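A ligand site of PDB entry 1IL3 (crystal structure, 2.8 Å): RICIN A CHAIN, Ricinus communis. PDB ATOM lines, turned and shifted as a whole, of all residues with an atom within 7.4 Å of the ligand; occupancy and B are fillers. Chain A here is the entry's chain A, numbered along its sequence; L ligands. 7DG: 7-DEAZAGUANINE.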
ATOM      1  N   ALA A  73     -11.900   6.473  19.131  1.00  0.00           N
ATOM      2  CA  ALA A  73     -11.633   7.842  19.537  1.00  0.00           C
ATOM      3  C   ALA A  73     -12.813   8.715  19.131  1.00  0.00           C
ATOM      4  O   ALA A  73     -13.095   8.900  17.937  1.00  0.00           O
ATOM      5  CB  ALA A  73     -10.363   8.342  18.876  1.00  0.00           C
ATOM      6  N   LEU A  74     -13.533   9.211  20.133  1.00  0.00           N
ATOM      7  CA  LEU A  74     -14.705  10.056  19.910  1.00  0.00           C
ATOM      8  C   LEU A  74     -14.402  11.516  20.188  1.00  0.00           C
ATOM      9  O   LEU A  74     -13.798  11.873  21.197  1.00  0.00           O
ATOM     10  CB  LEU A  74     -15.863   9.609  20.811  1.00  0.00           C
ATOM     11  CG  LEU A  74     -16.774   8.458  20.371  1.00  0.00           C
ATOM     12  CD1 LEU A  74     -17.628   8.902  19.204  1.00  0.00           C
ATOM     13  CD2 LEU A  74     -15.974   7.218  20.018  1.00  0.00           C
ATOM     14  N   ASN A  78     -18.748  16.719  18.776  1.00  0.00           N
ATOM     15  CA  ASN A  78     -19.804  16.226  17.885  1.00  0.00           C
ATOM     16  C   ASN A  78     -20.010  14.713  17.904  1.00  0.00           C
ATOM     17  O   ASN A  78     -20.775  14.199  17.092  1.00  0.00           O
ATOM     18  CB  ASN A  78     -19.523  16.680  16.450  1.00  0.00           C
ATOM     19  CG  ASN A  78     -18.207  16.135  15.909  1.00  0.00           C
ATOM     20  OD1 ASN A  78     -17.344  15.677  16.664  1.00  0.00           O
ATOM     21  ND2 ASN A  78     -18.045  16.199  14.593  1.00  0.00           N
ATOM     22  N   ALA A  79     -19.353  14.022  18.821  1.00  0.00           N
ATOM     23  CA  ALA A  79     -19.468  12.573  18.934  1.00  0.00           C
ATOM     24  C   ALA A  79     -19.111  11.902  17.607  1.00  0.00           C
ATOM     25  O   ALA A  79     -19.796  10.983  17.146  1.00  0.00           O
ATOM     26  CB  ALA A  79     -20.880  12.177  19.376  1.00  0.00           C
ATOM     27  N   TYR A  80     -18.023  12.363  16.997  1.00  0.00           N
ATOM     28  CA  TYR A  80     -17.560  11.844  15.715  1.00  0.00           C
ATOM     29  C   TYR A  80     -16.401  10.880  15.960  1.00  0.00           C
ATOM     30  O   TYR A  80     -15.449  11.219  16.685  1.00  0.00           O
ATOM     31  CB  TYR A  80     -17.088  13.002  14.841  1.00  0.00           C
ATOM     32  CG  TYR A  80     -16.893  12.697  13.368  1.00  0.00           C
ATOM     33  CD1 TYR A  80     -15.683  12.207  12.880  1.00  0.00           C
ATOM     34  CD2 TYR A  80     -17.927  12.941  12.454  1.00  0.00           C
ATOM     35  CE1 TYR A  80     -15.501  11.976  11.518  1.00  0.00           C
ATOM     36  CE2 TYR A  80     -17.745  12.710  11.093  1.00  0.00           C
ATOM     37  CZ  TYR A  80     -16.532  12.230  10.631  1.00  0.00           C
ATOM     38  OH  TYR A  80     -16.368  12.026   9.284  1.00  0.00           O
ATOM     39  N   VAL A  81     -16.481   9.688  15.384  1.00  0.00           N
ATOM     40  CA  VAL A  81     -15.424   8.703  15.536  1.00  0.00           C
ATOM     41  C   VAL A  81     -14.295   9.111  14.585  1.00  0.00           C
ATOM     42  O   VAL A  81     -14.427   8.984  13.366  1.00  0.00           O
ATOM     43  CB  VAL A  81     -15.918   7.273  15.179  1.00  0.00           C
ATOM     44  CG1 VAL A  81     -14.800   6.256  15.396  1.00  0.00           C
ATOM     45  CG2 VAL A  81     -17.125   6.915  16.030  1.00  0.00           C
ATOM     46  N   VAL A  82     -13.212   9.630  15.144  1.00  0.00           N
ATOM     47  CA  VAL A  82     -12.088  10.071  14.341  1.00  0.00           C
ATOM     48  C   VAL A  82     -11.094   8.956  13.994  1.00  0.00           C
ATOM     49  O   VAL A  82     -10.468   8.987  12.939  1.00  0.00           O
ATOM     50  CB  VAL A  82     -11.337  11.250  15.017  1.00  0.00           C
ATOM     51  CG1 VAL A  82     -12.279  12.436  15.187  1.00  0.00           C
ATOM     52  CG2 VAL A  82     -10.750  10.834  16.357  1.00  0.00           C
ATOM     53  N   GLY A  83     -10.956   7.980  14.882  1.00  0.00           N
ATOM     54  CA  GLY A  83     -10.030   6.883  14.635  1.00  0.00           C
ATOM     55  C   GLY A  83     -10.129   5.808  15.701  1.00  0.00           C
ATOM     56  O   GLY A  83     -11.011   5.861  16.559  1.00  0.00           O
ATOM     57  N   PHE A  93      -9.161   8.566  10.308  1.00  0.00           N
ATOM     58  CA  PHE A  93      -9.774   8.923   9.037  1.00  0.00           C
ATOM     59  C   PHE A  93      -9.093  10.199   8.556  1.00  0.00           C
ATOM     60  O   PHE A  93      -8.380  10.857   9.321  1.00  0.00           O
ATOM     61  CB  PHE A  93     -11.270   9.189   9.217  1.00  0.00           C
ATOM     62  CG  PHE A  93     -12.061   7.982   9.617  1.00  0.00           C
ATOM     63  CD1 PHE A  93     -12.162   6.881   8.767  1.00  0.00           C
ATOM     64  CD2 PHE A  93     -12.751   7.956  10.823  1.00  0.00           C
ATOM     65  CE1 PHE A  93     -12.937   5.781   9.111  1.00  0.00           C
ATOM     66  CE2 PHE A  93     -13.532   6.859  11.174  1.00  0.00           C
ATOM     67  CZ  PHE A  93     -13.625   5.779  10.323  1.00  0.00           C
ATOM     68  N   GLY A 120     -12.337   9.823   4.163  1.00  0.00           N
ATOM     69  CA  GLY A 120     -12.882  10.357   5.396  1.00  0.00           C
ATOM     70  C   GLY A 120     -13.851   9.377   6.022  1.00  0.00           C
ATOM     71  O   GLY A 120     -14.362   8.484   5.357  1.00  0.00           O
ATOM     72  N   GLY A 121     -14.135   9.564   7.314  1.00  0.00           N
ATOM     73  CA  GLY A 121     -15.041   8.674   8.014  1.00  0.00           C
ATOM     74  C   GLY A 121     -16.513   9.029   7.945  1.00  0.00           C
ATOM     75  O   GLY A 121     -17.318   8.456   8.675  1.00  0.00           O
ATOM     76  N   ASN A 122     -16.871   9.979   7.086  1.00  0.00           N
ATOM     77  CA  ASN A 122     -18.268  10.383   6.953  1.00  0.00           C
ATOM     78  C   ASN A 122     -19.090   9.344   6.189  1.00  0.00           C
ATOM     79  O   ASN A 122     -18.644   8.817   5.170  1.00  0.00           O
ATOM     80  CB  ASN A 122     -18.394  11.767   6.302  1.00  0.00           C
ATOM     81  CG  ASN A 122     -17.426  11.964   5.144  1.00  0.00           C
ATOM     82  OD1 ASN A 122     -17.530  11.318   4.113  1.00  0.00           O
ATOM     83  ND2 ASN A 122     -16.469  12.863   5.337  1.00  0.00           N
ATOM     84  N   TYR A 123     -20.274   9.049   6.719  1.00  0.00           N
ATOM     85  CA  TYR A 123     -21.194   8.064   6.152  1.00  0.00           C
ATOM     86  C   TYR A 123     -21.145   7.888   4.642  1.00  0.00           C
ATOM     87  O   TYR A 123     -20.961   6.769   4.166  1.00  0.00           O
ATOM     88  CB  TYR A 123     -22.629   8.365   6.576  1.00  0.00           C
ATOM     89  CG  TYR A 123     -22.982   7.949   7.991  1.00  0.00           C
ATOM     90  CD1 TYR A 123     -22.383   6.826   8.574  1.00  0.00           C
ATOM     91  CD2 TYR A 123     -23.919   8.655   8.738  1.00  0.00           C
ATOM     92  CE1 TYR A 123     -22.719   6.416   9.863  1.00  0.00           C
ATOM     93  CE2 TYR A 123     -24.268   8.255  10.025  1.00  0.00           C
ATOM     94  CZ  TYR A 123     -23.659   7.131  10.577  1.00  0.00           C
ATOM     95  OH  TYR A 123     -24.009   6.726  11.851  1.00  0.00           O
ATOM     96  N   ASP A 124     -21.313   8.970   3.894  1.00  0.00           N
ATOM     97  CA  ASP A 124     -21.300   8.923   2.439  1.00  0.00           C
ATOM     98  C   ASP A 124     -20.076   8.183   1.882  1.00  0.00           C
ATOM     99  O   ASP A 124     -20.219   7.307   1.031  1.00  0.00           O
ATOM    100  CB  ASP A 124     -21.383  10.335   1.840  1.00  0.00           C
ATOM    101  CG  ASP A 124     -20.287  11.262   2.348  1.00  0.00           C
ATOM    102  OD1 ASP A 124     -20.388  11.735   3.505  1.00  0.00           O
ATOM    103  OD2 ASP A 124     -19.319  11.521   1.591  1.00  0.00           O
ATOM    104  N   LEU A 126     -17.943   6.144   3.618  1.00  0.00           N
ATOM    105  CA  LEU A 126     -17.970   4.782   4.143  1.00  0.00           C
ATOM    106  C   LEU A 126     -18.944   3.841   3.430  1.00  0.00           C
ATOM    107  O   LEU A 126     -18.632   2.673   3.207  1.00  0.00           O
ATOM    108  CB  LEU A 126     -18.264   4.805   5.655  1.00  0.00           C
ATOM    109  CG  LEU A 126     -17.061   4.726   6.594  1.00  0.00           C
ATOM    110  CD1 LEU A 126     -15.937   5.638   6.141  1.00  0.00           C
ATOM    111  CD2 LEU A 126     -17.507   5.080   8.011  1.00  0.00           C
ATOM    112  N   ARG A 134     -26.505   2.201   4.683  1.00  0.00           N
ATOM    113  CA  ARG A 134     -26.837   1.915   6.078  1.00  0.00           C
ATOM    114  C   ARG A 134     -28.114   1.093   6.213  1.00  0.00           C
ATOM    115  O   ARG A 134     -28.167   0.150   7.005  1.00  0.00           O
ATOM    116  CB  ARG A 134     -26.972   3.214   6.868  1.00  0.00           C
ATOM    117  CG  ARG A 134     -25.659   3.923   7.179  1.00  0.00           C
ATOM    118  CD  ARG A 134     -25.904   5.316   7.728  1.00  0.00           C
ATOM    119  NE  ARG A 134     -26.445   6.212   6.707  1.00  0.00           N
ATOM    120  CZ  ARG A 134     -26.974   7.409   6.937  1.00  0.00           C
ATOM    121  NH1 ARG A 134     -27.060   7.881   8.176  1.00  0.00           N
ATOM    122  NH2 ARG A 134     -27.424   8.139   5.935  1.00  0.00           N
ATOM    123  N   PHE A 168     -17.185   0.069  10.749  1.00  0.00           N
ATOM    124  CA  PHE A 168     -17.185   1.426  11.275  1.00  0.00           C
ATOM    125  C   PHE A 168     -18.610   1.962  11.354  1.00  0.00           C
ATOM    126  O   PHE A 168     -19.019   2.467  12.400  1.00  0.00           O
ATOM    127  CB  PHE A 168     -16.328   2.361  10.405  1.00  0.00           C
ATOM    128  CG  PHE A 168     -14.892   2.454  10.844  1.00  0.00           C
ATOM    129  CD1 PHE A 168     -14.578   2.859  12.136  1.00  0.00           C
ATOM    130  CD2 PHE A 168     -13.856   2.173   9.960  1.00  0.00           C
ATOM    131  CE1 PHE A 168     -13.257   2.976  12.549  1.00  0.00           C
ATOM    132  CE2 PHE A 168     -12.528   2.288  10.365  1.00  0.00           C
ATOM    133  CZ  PHE A 168     -12.229   2.685  11.662  1.00  0.00           C
ATOM    134  N   ILE A 172     -20.485   3.143  14.699  1.00  0.00           N
ATOM    135  CA  ILE A 172     -20.888   4.547  14.778  1.00  0.00           C
ATOM    136  C   ILE A 172     -22.326   4.709  15.254  1.00  0.00           C
ATOM    137  O   ILE A 172     -22.594   5.409  16.234  1.00  0.00           O
ATOM    138  CB  ILE A 172     -20.726   5.255  13.415  1.00  0.00           C
ATOM    139  CG1 ILE A 172     -19.249   5.339  13.027  1.00  0.00           C
ATOM    140  CG2 ILE A 172     -21.316   6.657  13.472  1.00  0.00           C
ATOM    141  CD1 ILE A 172     -19.008   5.892  11.628  1.00  0.00           C
ATOM    142  N   GLN A 173     -23.253   4.057  14.550  1.00  0.00           N
ATOM    143  CA  GLN A 173     -24.670   4.120  14.878  1.00  0.00           C
ATOM    144  C   GLN A 173     -24.979   3.613  16.283  1.00  0.00           C
ATOM    145  O   GLN A 173     -25.691   4.273  17.035  1.00  0.00           O
ATOM    146  CB  GLN A 173     -25.480   3.343  13.842  1.00  0.00           C
ATOM    147  CG  GLN A 173     -25.370   3.871  12.423  1.00  0.00           C
ATOM    148  CD  GLN A 173     -26.205   3.082  11.440  1.00  0.00           C
ATOM    149  OE1 GLN A 173     -27.380   3.379  11.236  1.00  0.00           O
ATOM    150  NE2 GLN A 173     -25.615   2.063  10.834  1.00  0.00           N
ATOM    151  N   ILE A 175     -23.126   3.607  18.822  1.00  0.00           N
ATOM    152  CA  ILE A 175     -22.431   4.349  19.870  1.00  0.00           C
ATOM    153  C   ILE A 175     -22.702   5.847  19.777  1.00  0.00           C
ATOM    154  O   ILE A 175     -23.443   6.410  20.584  1.00  0.00           O
ATOM    155  CB  ILE A 175     -20.898   4.095  19.841  1.00  0.00           C
ATOM    156  CG1 ILE A 175     -20.600   2.606  20.048  1.00  0.00           C
ATOM    157  CG2 ILE A 175     -20.195   4.903  20.923  1.00  0.00           C
ATOM    158  CD1 ILE A 175     -19.136   2.247  19.959  1.00  0.00           C
ATOM    159  N   SER A 176     -22.118   6.495  18.773  1.00  0.00           N
ATOM    160  CA  SER A 176     -22.276   7.927  18.570  1.00  0.00           C
ATOM    161  C   SER A 176     -23.732   8.344  18.409  1.00  0.00           C
ATOM    162  O   SER A 176     -24.248   9.162  19.171  1.00  0.00           O
ATOM    163  CB  SER A 176     -21.461   8.385  17.357  1.00  0.00           C
ATOM    164  OG  SER A 176     -20.103   8.017  17.497  1.00  0.00           O
ATOM    165  N   GLU A 177     -24.411   7.721  17.453  1.00  0.00           N
ATOM    166  CA  GLU A 177     -25.812   8.033  17.187  1.00  0.00           C
ATOM    167  C   GLU A 177     -26.701   7.685  18.375  1.00  0.00           C
ATOM    168  O   GLU A 177     -27.676   8.403  18.660  1.00  0.00           O
ATOM    169  CB  GLU A 177     -26.291   7.324  15.928  1.00  0.00           C
ATOM    170  CG  GLU A 177     -25.497   7.652  14.652  1.00  0.00           C
ATOM    171  CD  GLU A 177     -25.723   9.063  14.124  1.00  0.00           C
ATOM    172  OE1 GLU A 177     -25.229   9.350  13.004  1.00  0.00           O
ATOM    173  OE2 GLU A 177     -26.368   9.894  14.797  1.00  0.00           O
ATOM    174  N   ARG A 180     -26.362  10.388  20.891  1.00  0.00           N
ATOM    175  CA  ARG A 180     -26.993  11.584  20.361  1.00  0.00           C
ATOM    176  C   ARG A 180     -28.497  11.543  20.517  1.00  0.00           C
ATOM    177  O   ARG A 180     -29.108  12.532  20.925  1.00  0.00           O
ATOM    178  CB  ARG A 180     -26.656  11.753  18.879  1.00  0.00           C
ATOM    179  CG  ARG A 180     -25.238  12.153  18.564  1.00  0.00           C
ATOM    180  CD  ARG A 180     -25.038  12.091  17.055  1.00  0.00           C
ATOM    181  NE  ARG A 180     -23.804  12.722  16.600  1.00  0.00           N
ATOM    182  CZ  ARG A 180     -23.459  12.815  15.320  1.00  0.00           C
ATOM    183  NH1 ARG A 180     -24.257  12.327  14.374  1.00  0.00           N
ATOM    184  NH2 ARG A 180     -22.336  13.429  14.984  1.00  0.00           N
ATOM    185  N   GLU A 208     -30.461  10.611  11.969  1.00  0.00           N
ATOM    186  CA  GLU A 208     -29.019  10.686  11.815  1.00  0.00           C
ATOM    187  C   GLU A 208     -28.657  11.774  10.804  1.00  0.00           C
ATOM    188  O   GLU A 208     -27.727  12.555  11.021  1.00  0.00           O
ATOM    189  CB  GLU A 208     -28.458   9.334  11.342  1.00  0.00           C
ATOM    190  CG  GLU A 208     -28.837   8.159  12.234  1.00  0.00           C
ATOM    191  CD  GLU A 208     -28.299   6.829  11.733  1.00  0.00           C
ATOM    192  OE1 GLU A 208     -28.230   6.621  10.513  1.00  0.00           O
ATOM    193  OE2 GLU A 208     -27.935   5.982  12.584  1.00  0.00           O
ATOM    194  N   TRP A 211     -29.457  15.436  12.543  1.00  0.00           N
ATOM    195  CA  TRP A 211     -28.902  15.836  13.839  1.00  0.00           C
ATOM    196  C   TRP A 211     -28.478  17.313  13.883  1.00  0.00           C
ATOM    197  O   TRP A 211     -28.977  18.079  14.708  1.00  0.00           O
ATOM    198  CB  TRP A 211     -27.717  14.946  14.228  1.00  0.00           C
ATOM    199  CG  TRP A 211     -27.184  15.214  15.597  1.00  0.00           C
ATOM    200  CD1 TRP A 211     -27.860  15.094  16.783  1.00  0.00           C
ATOM    201  CD2 TRP A 211     -25.864  15.656  15.937  1.00  0.00           C
ATOM    202  NE1 TRP A 211     -27.034  15.427  17.828  1.00  0.00           N
ATOM    203  CE2 TRP A 211     -25.806  15.779  17.340  1.00  0.00           C
ATOM    204  CE3 TRP A 211     -24.715  15.955  15.183  1.00  0.00           C
ATOM    205  CZ2 TRP A 211     -24.649  16.177  18.011  1.00  0.00           C
ATOM    206  CZ3 TRP A 211     -23.564  16.365  15.857  1.00  0.00           C
ATOM    207  CH2 TRP A 211     -23.536  16.466  17.257  1.00  0.00           C
HETATM  208  N9  7DG L   1     -20.631   9.940  14.324  1.00  0.00           N
HETATM  209  C8  7DG L   1     -21.885  10.265  13.960  1.00  0.00           C
HETATM  210  C7  7DG L   1     -21.980  10.318  12.566  1.00  0.00           C
HETATM  211  C5  7DG L   1     -20.708  10.001  12.090  1.00  0.00           C
HETATM  212  C6  7DG L   1     -20.147   9.888  10.815  1.00  0.00           C
HETATM  213  O6  7DG L   1     -20.761  10.070   9.791  1.00  0.00           O
HETATM  214  N1  7DG L   1     -18.838   9.538  10.741  1.00  0.00           N
HETATM  215  C2  7DG L   1     -18.077   9.316  11.838  1.00  0.00           C
HETATM  216  N2  7DG L   1     -16.782   8.976  11.763  1.00  0.00           N
HETATM  217  N3  7DG L   1     -18.590   9.428  13.086  1.00  0.00           N
HETATM  218  C4  7DG L   1     -19.895   9.774  13.206  1.00  0.00           C
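The backbone carbonyl oxygen of Gly 121 lies within hydrogen-bond range of a nitrogen (N1) of the ligand (2.8 Å).
A nitrogen (N3) of the ligand is in hydrogen-bond range of the backbone NH of Val 81, 3.1 Å away.
A nitrogen (N2) of the ligand sits at hydrogen-bond distance from the backbone carbonyl oxygen (O) of Val 81.
An oxygen (O6) of the ligand sits at hydrogen-bond distance from the backbone NH (N) of Tyr 123 (3.3 Å).
O of Ala 79 sits at hydrogen-bond distance from OG of Ser 176, 3.0 Å away.
The guanidinium group of Arg 180 lies within salt-bridge range of the side-chain carboxylate of Glu 177 (3.2 Å).
The guanidinium group of Arg 180 sits at hydrogen-bond distance from the backbone carbonyl oxygen of Asn 78, at 2.7 Å.
The side-chain hydroxyl of Tyr 80 lies within hydrogen-bond range of the backbone NH of Asn 122 (3.0 Å).
The backbone NH (N) of Tyr 80 lies close to the side-chain amide oxygen (OD1) of Asn 78.
The backbone carbonyl oxygen of Ile 172 is in hydrogen-bond range of the backbone NH of Glu 177 (3.2 Å).
The side-chain carboxylate (OD1) of Asp 124 lies close to the side-chain amide oxygen (OD1) of Asn 122, 3.0 Å away.
N of Phe 93 lies within hydrogen-bond range of O of Val 82 (3.0 Å).
The backbone carbonyl oxygen (O) of Ala 79 lies close to a nitrogen (N9) of the ligand, 3.1 Å away.
Tyr 80 touches the ligand (CE1 to N2, 3.3 Å).
Phe 93 touches the ligand.
Asn 122 touches the ligand (CA to O6, 3.8 Å).
Ile 172 touches the ligand (CG2 to C4, 3.4 Å).
CB of Ser 176 touches N9 of the ligand, 3.5 Å away.
Glu 177 touches the ligand.
Arg 180 touches the ligand (NH1 to C8, 3.2 Å).
The nearest printed residue that does not touch the ligand is Val 82 (5.0 Å).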
